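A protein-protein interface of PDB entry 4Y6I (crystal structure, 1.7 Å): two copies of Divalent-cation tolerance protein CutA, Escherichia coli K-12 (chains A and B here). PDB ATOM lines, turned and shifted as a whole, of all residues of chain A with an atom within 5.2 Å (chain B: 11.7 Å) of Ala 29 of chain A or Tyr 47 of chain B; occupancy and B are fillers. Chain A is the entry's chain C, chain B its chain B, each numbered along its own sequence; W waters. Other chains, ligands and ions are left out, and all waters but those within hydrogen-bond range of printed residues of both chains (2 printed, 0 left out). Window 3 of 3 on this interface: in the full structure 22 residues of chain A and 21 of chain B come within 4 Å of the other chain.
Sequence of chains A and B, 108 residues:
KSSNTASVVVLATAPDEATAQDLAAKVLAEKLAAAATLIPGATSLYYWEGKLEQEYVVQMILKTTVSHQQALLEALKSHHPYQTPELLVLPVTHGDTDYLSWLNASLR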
ATOM      1  N   ALA A  24      18.961   3.044  14.914  1.00  0.00           N
ATOM      2  CA  ALA A  24      18.926   3.190  13.469  1.00  0.00           C
ATOM      3  C   ALA A  24      17.479   3.240  12.988  1.00  0.00           C
ATOM      4  O   ALA A  24      17.115   4.113  12.203  1.00  0.00           O
ATOM      5  CB  ALA A  24      19.689   2.052  12.783  1.00  0.00           C
ATOM      6  N   ALA A  25      16.650   2.319  13.484  1.00  0.00           N
ATOM      7  CA  ALA A  25      15.272   2.245  13.017  1.00  0.00           C
ATOM      8  C   ALA A  25      14.534   3.552  13.285  1.00  0.00           C
ATOM      9  O   ALA A  25      13.806   4.036  12.428  1.00  0.00           O
ATOM     10  CB  ALA A  25      14.535   1.055  13.661  1.00  0.00           C
ATOM     11  N   LYS A  26      14.750   4.128  14.469  1.00  0.00           N
ATOM     12  CA  LYS A  26      14.089   5.374  14.860  1.00  0.00           C
ATOM     13  C   LYS A  26      14.494   6.563  13.981  1.00  0.00           C
ATOM     14  O   LYS A  26      13.643   7.261  13.431  1.00  0.00           O
ATOM     15  CB  LYS A  26      14.348   5.668  16.340  1.00  0.00           C
ATOM     16  CG  LYS A  26      13.460   4.843  17.269  1.00  0.00           C
ATOM     17  CD  LYS A  26      13.888   4.942  18.717  1.00  0.00           C
ATOM     18  CE  LYS A  26      12.808   4.368  19.625  1.00  0.00           C
ATOM     19  NZ  LYS A  26      13.304   4.214  21.020  1.00  0.00           N
ATOM     20  N   VAL A  27      15.797   6.781  13.825  1.00  0.00           N
ATOM     21  CA  VAL A  27      16.250   7.923  13.048  1.00  0.00           C
ATOM     22  C   VAL A  27      15.989   7.761  11.552  1.00  0.00           C
ATOM     23  O   VAL A  27      15.815   8.750  10.855  1.00  0.00           O
ATOM     24  CB  VAL A  27      17.729   8.282  13.341  1.00  0.00           C
ATOM     25  CG1 VAL A  27      17.911   8.534  14.844  1.00  0.00           C
ATOM     26  CG2 VAL A  27      18.683   7.205  12.828  1.00  0.00           C
ATOM     27  N   LEU A  28      15.936   6.519  11.069  1.00  0.00           N
ATOM     28  CA  LEU A  28      15.577   6.283   9.671  1.00  0.00           C
ATOM     29  C   LEU A  28      14.084   6.590   9.456  1.00  0.00           C
ATOM     30  O   LEU A  28      13.713   7.251   8.487  1.00  0.00           O
ATOM     31  CB  LEU A  28      15.920   4.845   9.252  1.00  0.00           C
ATOM     32  CG  LEU A  28      17.414   4.533   9.088  1.00  0.00           C
ATOM     33  CD1 LEU A  28      17.579   3.047   8.887  1.00  0.00           C
ATOM     34  CD2 LEU A  28      18.055   5.283   7.939  1.00  0.00           C
ATOM     35  N   ALA A  29      13.241   6.138  10.378  1.00  0.00           N
ATOM     36  CA  ALA A  29      11.794   6.407  10.274  1.00  0.00           C
ATOM     37  C   ALA A  29      11.480   7.909  10.342  1.00  0.00           C
ATOM     38  O   ALA A  29      10.547   8.397   9.672  1.00  0.00           O
ATOM     39  CB  ALA A  29      11.031   5.649  11.354  1.00  0.00           C
ATOM     40  N   GLU A  30      12.270   8.636  11.133  1.00  0.00           N
ATOM     41  CA  GLU A  30      12.117  10.084  11.290  1.00  0.00           C
ATOM     42  C   GLU A  30      12.778  10.876  10.148  1.00  0.00           C
ATOM     43  O   GLU A  30      12.725  12.115  10.122  1.00  0.00           O
ATOM     44  CB  GLU A  30      12.639  10.530  12.660  1.00  0.00           C
ATOM     45  CG  GLU A  30      11.816   9.948  13.805  1.00  0.00           C
ATOM     46  CD  GLU A  30      12.281  10.351  15.187  1.00  0.00           C
ATOM     47  OE1 GLU A  30      13.454  10.775  15.360  1.00  0.00           O
ATOM     48  OE2 GLU A  30      11.452  10.221  16.122  1.00  0.00           O
ATOM     49  N   LYS A  31      13.377  10.147   9.203  1.00  0.00           N
ATOM     50  CA  LYS A  31      14.096  10.724   8.062  1.00  0.00           C
ATOM     51  C   LYS A  31      15.159  11.742   8.492  1.00  0.00           C
ATOM     52  O   LYS A  31      15.284  12.824   7.914  1.00  0.00           O
ATOM     53  CB  LYS A  31      13.119  11.327   7.039  1.00  0.00           C
ATOM     54  CG  LYS A  31      12.022  10.352   6.609  1.00  0.00           C
ATOM     55  CD  LYS A  31      10.891  11.103   5.894  1.00  0.00           C
ATOM     56  CE  LYS A  31      11.126  11.222   4.409  1.00  0.00           C
ATOM     57  NZ  LYS A  31      10.894   9.935   3.691  1.00  0.00           N
ATOM     58  N   ALA A  34      19.700   8.706   6.149  1.00  0.00           N
ATOM     59  CA  ALA A  34      19.317   7.942   4.963  1.00  0.00           C
ATOM     60  C   ALA A  34      19.614   6.446   5.106  1.00  0.00           C
ATOM     61  O   ALA A  34      18.914   5.595   4.534  1.00  0.00           O
ATOM     62  CB  ALA A  34      20.023   8.505   3.731  1.00  0.00           C
ATOM     63  N   TRP A 102      20.257  10.122  -3.991  1.00  0.00           N
ATOM     64  CA  TRP A 102      19.325   9.294  -3.230  1.00  0.00           C
ATOM     65  C   TRP A 102      19.339   9.685  -1.748  1.00  0.00           C
ATOM     66  O   TRP A 102      18.284   9.796  -1.119  1.00  0.00           O
ATOM     67  CB  TRP A 102      19.656   7.804  -3.397  1.00  0.00           C
ATOM     68  CG  TRP A 102      18.886   6.942  -2.452  1.00  0.00           C
ATOM     69  CD1 TRP A 102      17.604   6.495  -2.604  1.00  0.00           C
ATOM     70  CD2 TRP A 102      19.335   6.448  -1.179  1.00  0.00           C
ATOM     71  NE1 TRP A 102      17.225   5.748  -1.510  1.00  0.00           N
ATOM     72  CE2 TRP A 102      18.269   5.703  -0.619  1.00  0.00           C
ATOM     73  CE3 TRP A 102      20.536   6.557  -0.462  1.00  0.00           C
ATOM     74  CZ2 TRP A 102      18.371   5.063   0.627  1.00  0.00           C
ATOM     75  CZ3 TRP A 102      20.634   5.927   0.777  1.00  0.00           C
ATOM     76  CH2 TRP A 102      19.561   5.191   1.310  1.00  0.00           C
ATOM     77  N   THR B  43      25.575  -5.026   9.018  1.00  0.00           N
ATOM     78  CA  THR B  43      24.194  -4.898   8.544  1.00  0.00           C
ATOM     79  C   THR B  43      23.934  -3.460   8.097  1.00  0.00           C
ATOM     80  O   THR B  43      24.311  -2.521   8.802  1.00  0.00           O
ATOM     81  CB  THR B  43      23.191  -5.304   9.661  1.00  0.00           C
ATOM     82  OG1 THR B  43      23.356  -6.700   9.949  1.00  0.00           O
ATOM     83  CG2 THR B  43      21.756  -5.065   9.231  1.00  0.00           C
ATOM     84  N   SER B  44      23.310  -3.291   6.932  1.00  0.00           N
ATOM     85  CA  SER B  44      22.883  -1.969   6.475  1.00  0.00           C
ATOM     86  C   SER B  44      21.373  -1.862   6.547  1.00  0.00           C
ATOM     87  O   SER B  44      20.662  -2.754   6.069  1.00  0.00           O
ATOM     88  CB  SER B  44      23.358  -1.685   5.052  1.00  0.00           C
ATOM     89  OG  SER B  44      22.813  -0.466   4.547  1.00  0.00           O
ATOM     90  N   LEU B  45      20.910  -0.785   7.182  1.00  0.00           N
ATOM     91  CA  LEU B  45      19.481  -0.474   7.252  1.00  0.00           C
ATOM     92  C   LEU B  45      19.194   0.803   6.482  1.00  0.00           C
ATOM     93  O   LEU B  45      19.954   1.773   6.552  1.00  0.00           O
ATOM     94  CB  LEU B  45      19.002  -0.325   8.702  1.00  0.00           C
ATOM     95  CG  LEU B  45      19.048  -1.532   9.640  1.00  0.00           C
ATOM     96  CD1 LEU B  45      20.429  -1.697  10.224  1.00  0.00           C
ATOM     97  CD2 LEU B  45      18.023  -1.357  10.752  1.00  0.00           C
ATOM     98  N   TYR B  46      18.095   0.792   5.732  1.00  0.00           N
ATOM     99  CA  TYR B  46      17.682   1.950   4.961  1.00  0.00           C
ATOM    100  C   TYR B  46      16.266   1.701   4.489  1.00  0.00           C
ATOM    101  O   TYR B  46      15.832   0.550   4.442  1.00  0.00           O
ATOM    102  CB  TYR B  46      18.620   2.185   3.760  1.00  0.00           C
ATOM    103  CG  TYR B  46      18.710   1.009   2.808  1.00  0.00           C
ATOM    104  CD1 TYR B  46      17.888   0.948   1.680  1.00  0.00           C
ATOM    105  CD2 TYR B  46      19.597  -0.044   3.043  1.00  0.00           C
ATOM    106  CE1 TYR B  46      17.955  -0.126   0.808  1.00  0.00           C
ATOM    107  CE2 TYR B  46      19.668  -1.135   2.165  1.00  0.00           C
ATOM    108  CZ  TYR B  46      18.839  -1.153   1.051  1.00  0.00           C
ATOM    109  OH  TYR B  46      18.872  -2.210   0.163  1.00  0.00           O
ATOM    110  N   TYR B  47      15.549   2.770   4.160  1.00  0.00           N
ATOM    111  CA  TYR B  47      14.239   2.630   3.535  1.00  0.00           C
ATOM    112  C   TYR B  47      14.315   2.573   2.023  1.00  0.00           C
ATOM    113  O   TYR B  47      15.054   3.330   1.393  1.00  0.00           O
ATOM    114  CB  TYR B  47      13.312   3.769   3.954  1.00  0.00           C
ATOM    115  CG  TYR B  47      12.634   3.501   5.265  1.00  0.00           C
ATOM    116  CD1 TYR B  47      11.412   2.831   5.310  1.00  0.00           C
ATOM    117  CD2 TYR B  47      13.217   3.909   6.469  1.00  0.00           C
ATOM    118  CE1 TYR B  47      10.789   2.572   6.522  1.00  0.00           C
ATOM    119  CE2 TYR B  47      12.602   3.655   7.680  1.00  0.00           C
ATOM    120  CZ  TYR B  47      11.383   2.987   7.697  1.00  0.00           C
ATOM    121  OH  TYR B  47      10.774   2.741   8.909  1.00  0.00           O
ATOM    122  N   TRP B  48      13.528   1.673   1.447  1.00  0.00           N
ATOM    123  CA  TRP B  48      13.345   1.645   0.010  1.00  0.00           C
ATOM    124  C   TRP B  48      11.855   1.432  -0.243  1.00  0.00           C
ATOM    125  O   TRP B  48      11.294   0.413   0.172  1.00  0.00           O
ATOM    126  CB  TRP B  48      14.188   0.538  -0.610  1.00  0.00           C
ATOM    127  CG  TRP B  48      14.160   0.547  -2.103  1.00  0.00           C
ATOM    128  CD1 TRP B  48      14.921   1.322  -2.933  1.00  0.00           C
ATOM    129  CD2 TRP B  48      13.318  -0.248  -2.947  1.00  0.00           C
ATOM    130  NE1 TRP B  48      14.611   1.048  -4.247  1.00  0.00           N
ATOM    131  CE2 TRP B  48      13.630   0.090  -4.284  1.00  0.00           C
ATOM    132  CE3 TRP B  48      12.338  -1.221  -2.704  1.00  0.00           C
ATOM    133  CZ2 TRP B  48      12.989  -0.510  -5.381  1.00  0.00           C
ATOM    134  CZ3 TRP B  48      11.698  -1.821  -3.797  1.00  0.00           C
ATOM    135  CH2 TRP B  48      12.030  -1.459  -5.118  1.00  0.00           C
ATOM    136  N   GLU B  49      11.230   2.412  -0.895  1.00  0.00           N
ATOM    137  CA  GLU B  49       9.776   2.436  -1.119  1.00  0.00           C
ATOM    138  C   GLU B  49       8.981   2.006   0.114  1.00  0.00           C
ATOM    139  O   GLU B  49       8.160   1.081   0.061  1.00  0.00           O
ATOM    140  CB  GLU B  49       9.397   1.605  -2.344  1.00  0.00           C
ATOM    141  CG  GLU B  49       9.895   2.214  -3.642  1.00  0.00           C
ATOM    142  CD  GLU B  49       9.632   1.344  -4.849  1.00  0.00           C
ATOM    143  OE1 GLU B  49       9.245   0.165  -4.685  1.00  0.00           O
ATOM    144  OE2 GLU B  49       9.821   1.851  -5.976  1.00  0.00           O
ATOM    145  N   GLY B  50       9.251   2.679   1.224  1.00  0.00           N
ATOM    146  CA  GLY B  50       8.508   2.482   2.469  1.00  0.00           C
ATOM    147  C   GLY B  50       8.839   1.237   3.266  1.00  0.00           C
ATOM    148  O   GLY B  50       8.272   1.014   4.331  1.00  0.00           O
ATOM    149  N   LYS B  51       9.756   0.425   2.756  1.00  0.00           N
ATOM    150  CA  LYS B  51      10.162  -0.802   3.423  1.00  0.00           C
ATOM    151  C   LYS B  51      11.507  -0.589   4.119  1.00  0.00           C
ATOM    152  O   LYS B  51      12.449  -0.111   3.500  1.00  0.00           O
ATOM    153  CB  LYS B  51      10.245  -1.919   2.385  1.00  0.00           C
ATOM    154  CG  LYS B  51      11.050  -3.150   2.753  1.00  0.00           C
ATOM    155  CD  LYS B  51      10.701  -4.340   1.828  1.00  0.00           C
ATOM    156  CE  LYS B  51      10.126  -3.884   0.486  1.00  0.00           C
ATOM    157  NZ  LYS B  51      11.150  -3.291  -0.418  1.00  0.00           N
ATOM    158  N   LEU B  52      11.589  -0.945   5.397  1.00  0.00           N
ATOM    159  CA  LEU B  52      12.873  -0.916   6.090  1.00  0.00           C
ATOM    160  C   LEU B  52      13.658  -2.139   5.675  1.00  0.00           C
ATOM    161  O   LEU B  52      13.360  -3.256   6.111  1.00  0.00           O
ATOM    162  CB  LEU B  52      12.717  -0.863   7.613  1.00  0.00           C
ATOM    163  CG  LEU B  52      14.025  -0.844   8.429  1.00  0.00           C
ATOM    164  CD1 LEU B  52      14.835   0.437   8.161  1.00  0.00           C
ATOM    165  CD2 LEU B  52      13.726  -0.989   9.903  1.00  0.00           C
ATOM    166  N   GLU B  53      14.637  -1.912   4.807  1.00  0.00           N
ATOM    167  CA  GLU B  53      15.500  -2.983   4.326  1.00  0.00           C
ATOM    168  C   GLU B  53      16.584  -3.259   5.365  1.00  0.00           C
ATOM    169  O   GLU B  53      17.064  -2.345   6.045  1.00  0.00           O
ATOM    170  CB  GLU B  53      16.129  -2.616   2.975  1.00  0.00           C
ATOM    171  CG  GLU B  53      15.135  -2.247   1.867  1.00  0.00           C
ATOM    172  CD  GLU B  53      14.552  -3.457   1.143  1.00  0.00           C
ATOM    173  OE1 GLU B  53      14.222  -4.459   1.812  1.00  0.00           O
ATOM    174  OE2 GLU B  53      14.417  -3.398  -0.100  1.00  0.00           O
ATOM    175  N   GLN B  54      16.951  -4.525   5.498  1.00  0.00           N
ATOM    176  CA  GLN B  54      18.014  -4.920   6.394  1.00  0.00           C
ATOM    177  C   GLN B  54      18.871  -5.908   5.626  1.00  0.00           C
ATOM    178  O   GLN B  54      18.476  -7.061   5.432  1.00  0.00           O
ATOM    179  CB  GLN B  54      17.457  -5.544   7.669  1.00  0.00           C
ATOM    180  CG  GLN B  54      18.524  -5.891   8.693  1.00  0.00           C
ATOM    181  CD  GLN B  54      17.981  -6.005  10.108  1.00  0.00           C
ATOM    182  OE1 GLN B  54      17.091  -5.249  10.513  1.00  0.00           O
ATOM    183  NE2 GLN B  54      18.527  -6.950  10.875  1.00  0.00           N
ATOM    184  N   GLU B  55      20.020  -5.443   5.156  1.00  0.00           N
ATOM    185  CA  GLU B  55      20.876  -6.301   4.346  1.00  0.00           C
ATOM    186  C   GLU B  55      22.245  -6.500   4.970  1.00  0.00           C
ATOM    187  O   GLU B  55      22.800  -5.599   5.604  1.00  0.00           O
ATOM    188  CB  GLU B  55      20.971  -5.800   2.898  1.00  0.00           C
ATOM    189  CG  GLU B  55      21.623  -4.434   2.693  1.00  0.00           C
ATOM    190  CD  GLU B  55      22.071  -4.189   1.251  1.00  0.00           C
ATOM    191  OE1 GLU B  55      22.497  -5.149   0.569  1.00  0.00           O
ATOM    192  OE2 GLU B  55      22.023  -3.026   0.801  1.00  0.00           O
ATOM    193  N   GLN B  83      22.952  -0.580  -8.470  1.00  0.00           N
ATOM    194  CA  GLN B  83      22.805   0.689  -9.195  1.00  0.00           C
ATOM    195  C   GLN B  83      23.069   1.956  -8.370  1.00  0.00           C
ATOM    196  O   GLN B  83      23.366   3.013  -8.930  1.00  0.00           O
ATOM    197  CB  GLN B  83      21.417   0.783  -9.860  1.00  0.00           C
ATOM    198  CG  GLN B  83      20.244   0.959  -8.890  1.00  0.00           C
ATOM    199  CD  GLN B  83      18.882   1.019  -9.581  1.00  0.00           C
ATOM    200  OE1 GLN B  83      18.749   0.691 -10.765  1.00  0.00           O
ATOM    201  NE2 GLN B  83      17.862   1.434  -8.837  1.00  0.00           N
ATOM    202  N   THR B  84      22.960   1.861  -7.051  1.00  0.00           N
ATOM    203  CA  THR B  84      23.126   3.035  -6.192  1.00  0.00           C
ATOM    204  C   THR B  84      24.102   2.692  -5.055  1.00  0.00           C
ATOM    205  O   THR B  84      23.703   2.623  -3.896  1.00  0.00           O
ATOM    206  CB  THR B  84      21.756   3.519  -5.650  1.00  0.00           C
ATOM    207  OG1 THR B  84      20.849   3.711  -6.749  1.00  0.00           O
ATOM    208  CG2 THR B  84      21.891   4.835  -4.891  1.00  0.00           C
ATOM    209  N   GLU B  86      26.860   2.598  -2.139  1.00  0.00           N
ATOM    210  CA  GLU B  86      27.306   3.495  -1.076  1.00  0.00           C
ATOM    211  C   GLU B  86      28.819   3.663  -1.135  1.00  0.00           C
ATOM    212  O   GLU B  86      29.571   2.823  -0.612  1.00  0.00           O
ATOM    213  CB  GLU B  86      26.876   2.959   0.286  1.00  0.00           C
ATOM    214  CG  GLU B  86      27.233   3.907   1.423  1.00  0.00           C
ATOM    215  CD  GLU B  86      27.062   3.290   2.786  1.00  0.00           C
ATOM    216  OE1 GLU B  86      26.116   2.488   2.979  1.00  0.00           O
ATOM    217  OE2 GLU B  86      27.885   3.618   3.670  1.00  0.00           O
HETATM  218  O   HOH W   1      12.362   2.293  10.929  1.00  0.00           O
HETATM  219  O   HOH W   2      16.257   5.562   4.271  1.00  0.00           O
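No position is printed for both chains. Of the 8 pairs that touch across the chains among the printed residues, none has its exchanged pair printed and touching as well.
Hydrophobic or aromatic side chains of chain A within 4 Å of the printed part of chain B: Leu 28, Ala 29 and Trp 102. Hydrophobic or aromatic side chains of chain B within 4 Å of the printed part of chain A: Leu 45, Tyr 46, Tyr 47 and Leu 52. Among the printed residues, 8 pairs touch across the chains. Among the printed residues, no Asp or Glu carboxylate lies within 4 Å of a Lys or Arg side-chain nitrogen of the other chain.
Among the printed residues, pairs that only touch across the chains: Ala 34 of chain A with Tyr 46 of chain B (3.5 Å), Leu 28 of chain A with Leu 45 of chain B (3.6 Å), Ala 29 of chain A with Tyr 47 of chain B (3.7 Å), Leu 28 of chain A with Tyr 47 of chain B (3.7 Å), Trp 102 of chain A with Tyr 47 of chain B (3.8 Å), Leu 28 of chain A with Leu 52 of chain B (3.9 Å), Leu 28 of chain A with Tyr 46 of chain B (3.9 Å) and Trp 102 of chain A with Tyr 46 of chain B (3.99 Å).
Of the printed residues of chain B, Ala 29 of chain A touches Tyr 47. Tyr 47 of chain B touches three residues of chain A. Ala 25 of chain A touches none of the printed residues of chain B. No residue of chain B comes within 4 Å of Val 27 of chain A. Of the printed residues of chain B, Leu 28 of chain A touches Leu 45 (3.6 Å), Tyr 46 (3.9 Å), Tyr 47 (3.7 Å) and Leu 52 (3.9 Å). Printed residues of chain A within 4 Å of Tyr 46 of chain B: Leu 28 (3.9 Å), Ala 34 (3.5 Å) and Trp 102 (3.99 Å). Of the printed residues of chain B, Trp 102 of chain A touches Tyr 46 (3.99 Å) and Tyr 47 (3.8 Å). Ala 24 of chain A touches none of the printed residues of chain B. The nearest residue of chain A that does not touch Tyr 47 of chain B is Ala 34 of chain A (4.4 Å).
Water W1 lies within hydrogen-bond range of the side-chain hydroxyl (OH) of Tyr 47 of chain B and the backbone carbonyl oxygen (O) of Ala 25 of chain A. Water W2 bridges O of Ala 34 of chain A (2.7 Å) and N of Tyr 47 of chain B (2.9 Å).
The backbone NH of Glu 53 of chain B lies within hydrogen-bond range of the backbone carbonyl oxygen of Tyr 46 of chain B (2.8 Å). The side-chain hydroxyl (OH) of Tyr 46 of chain B sits close to the side-chain carboxylate (OE2) of Glu 55 of chain B, at 3.3 Å.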
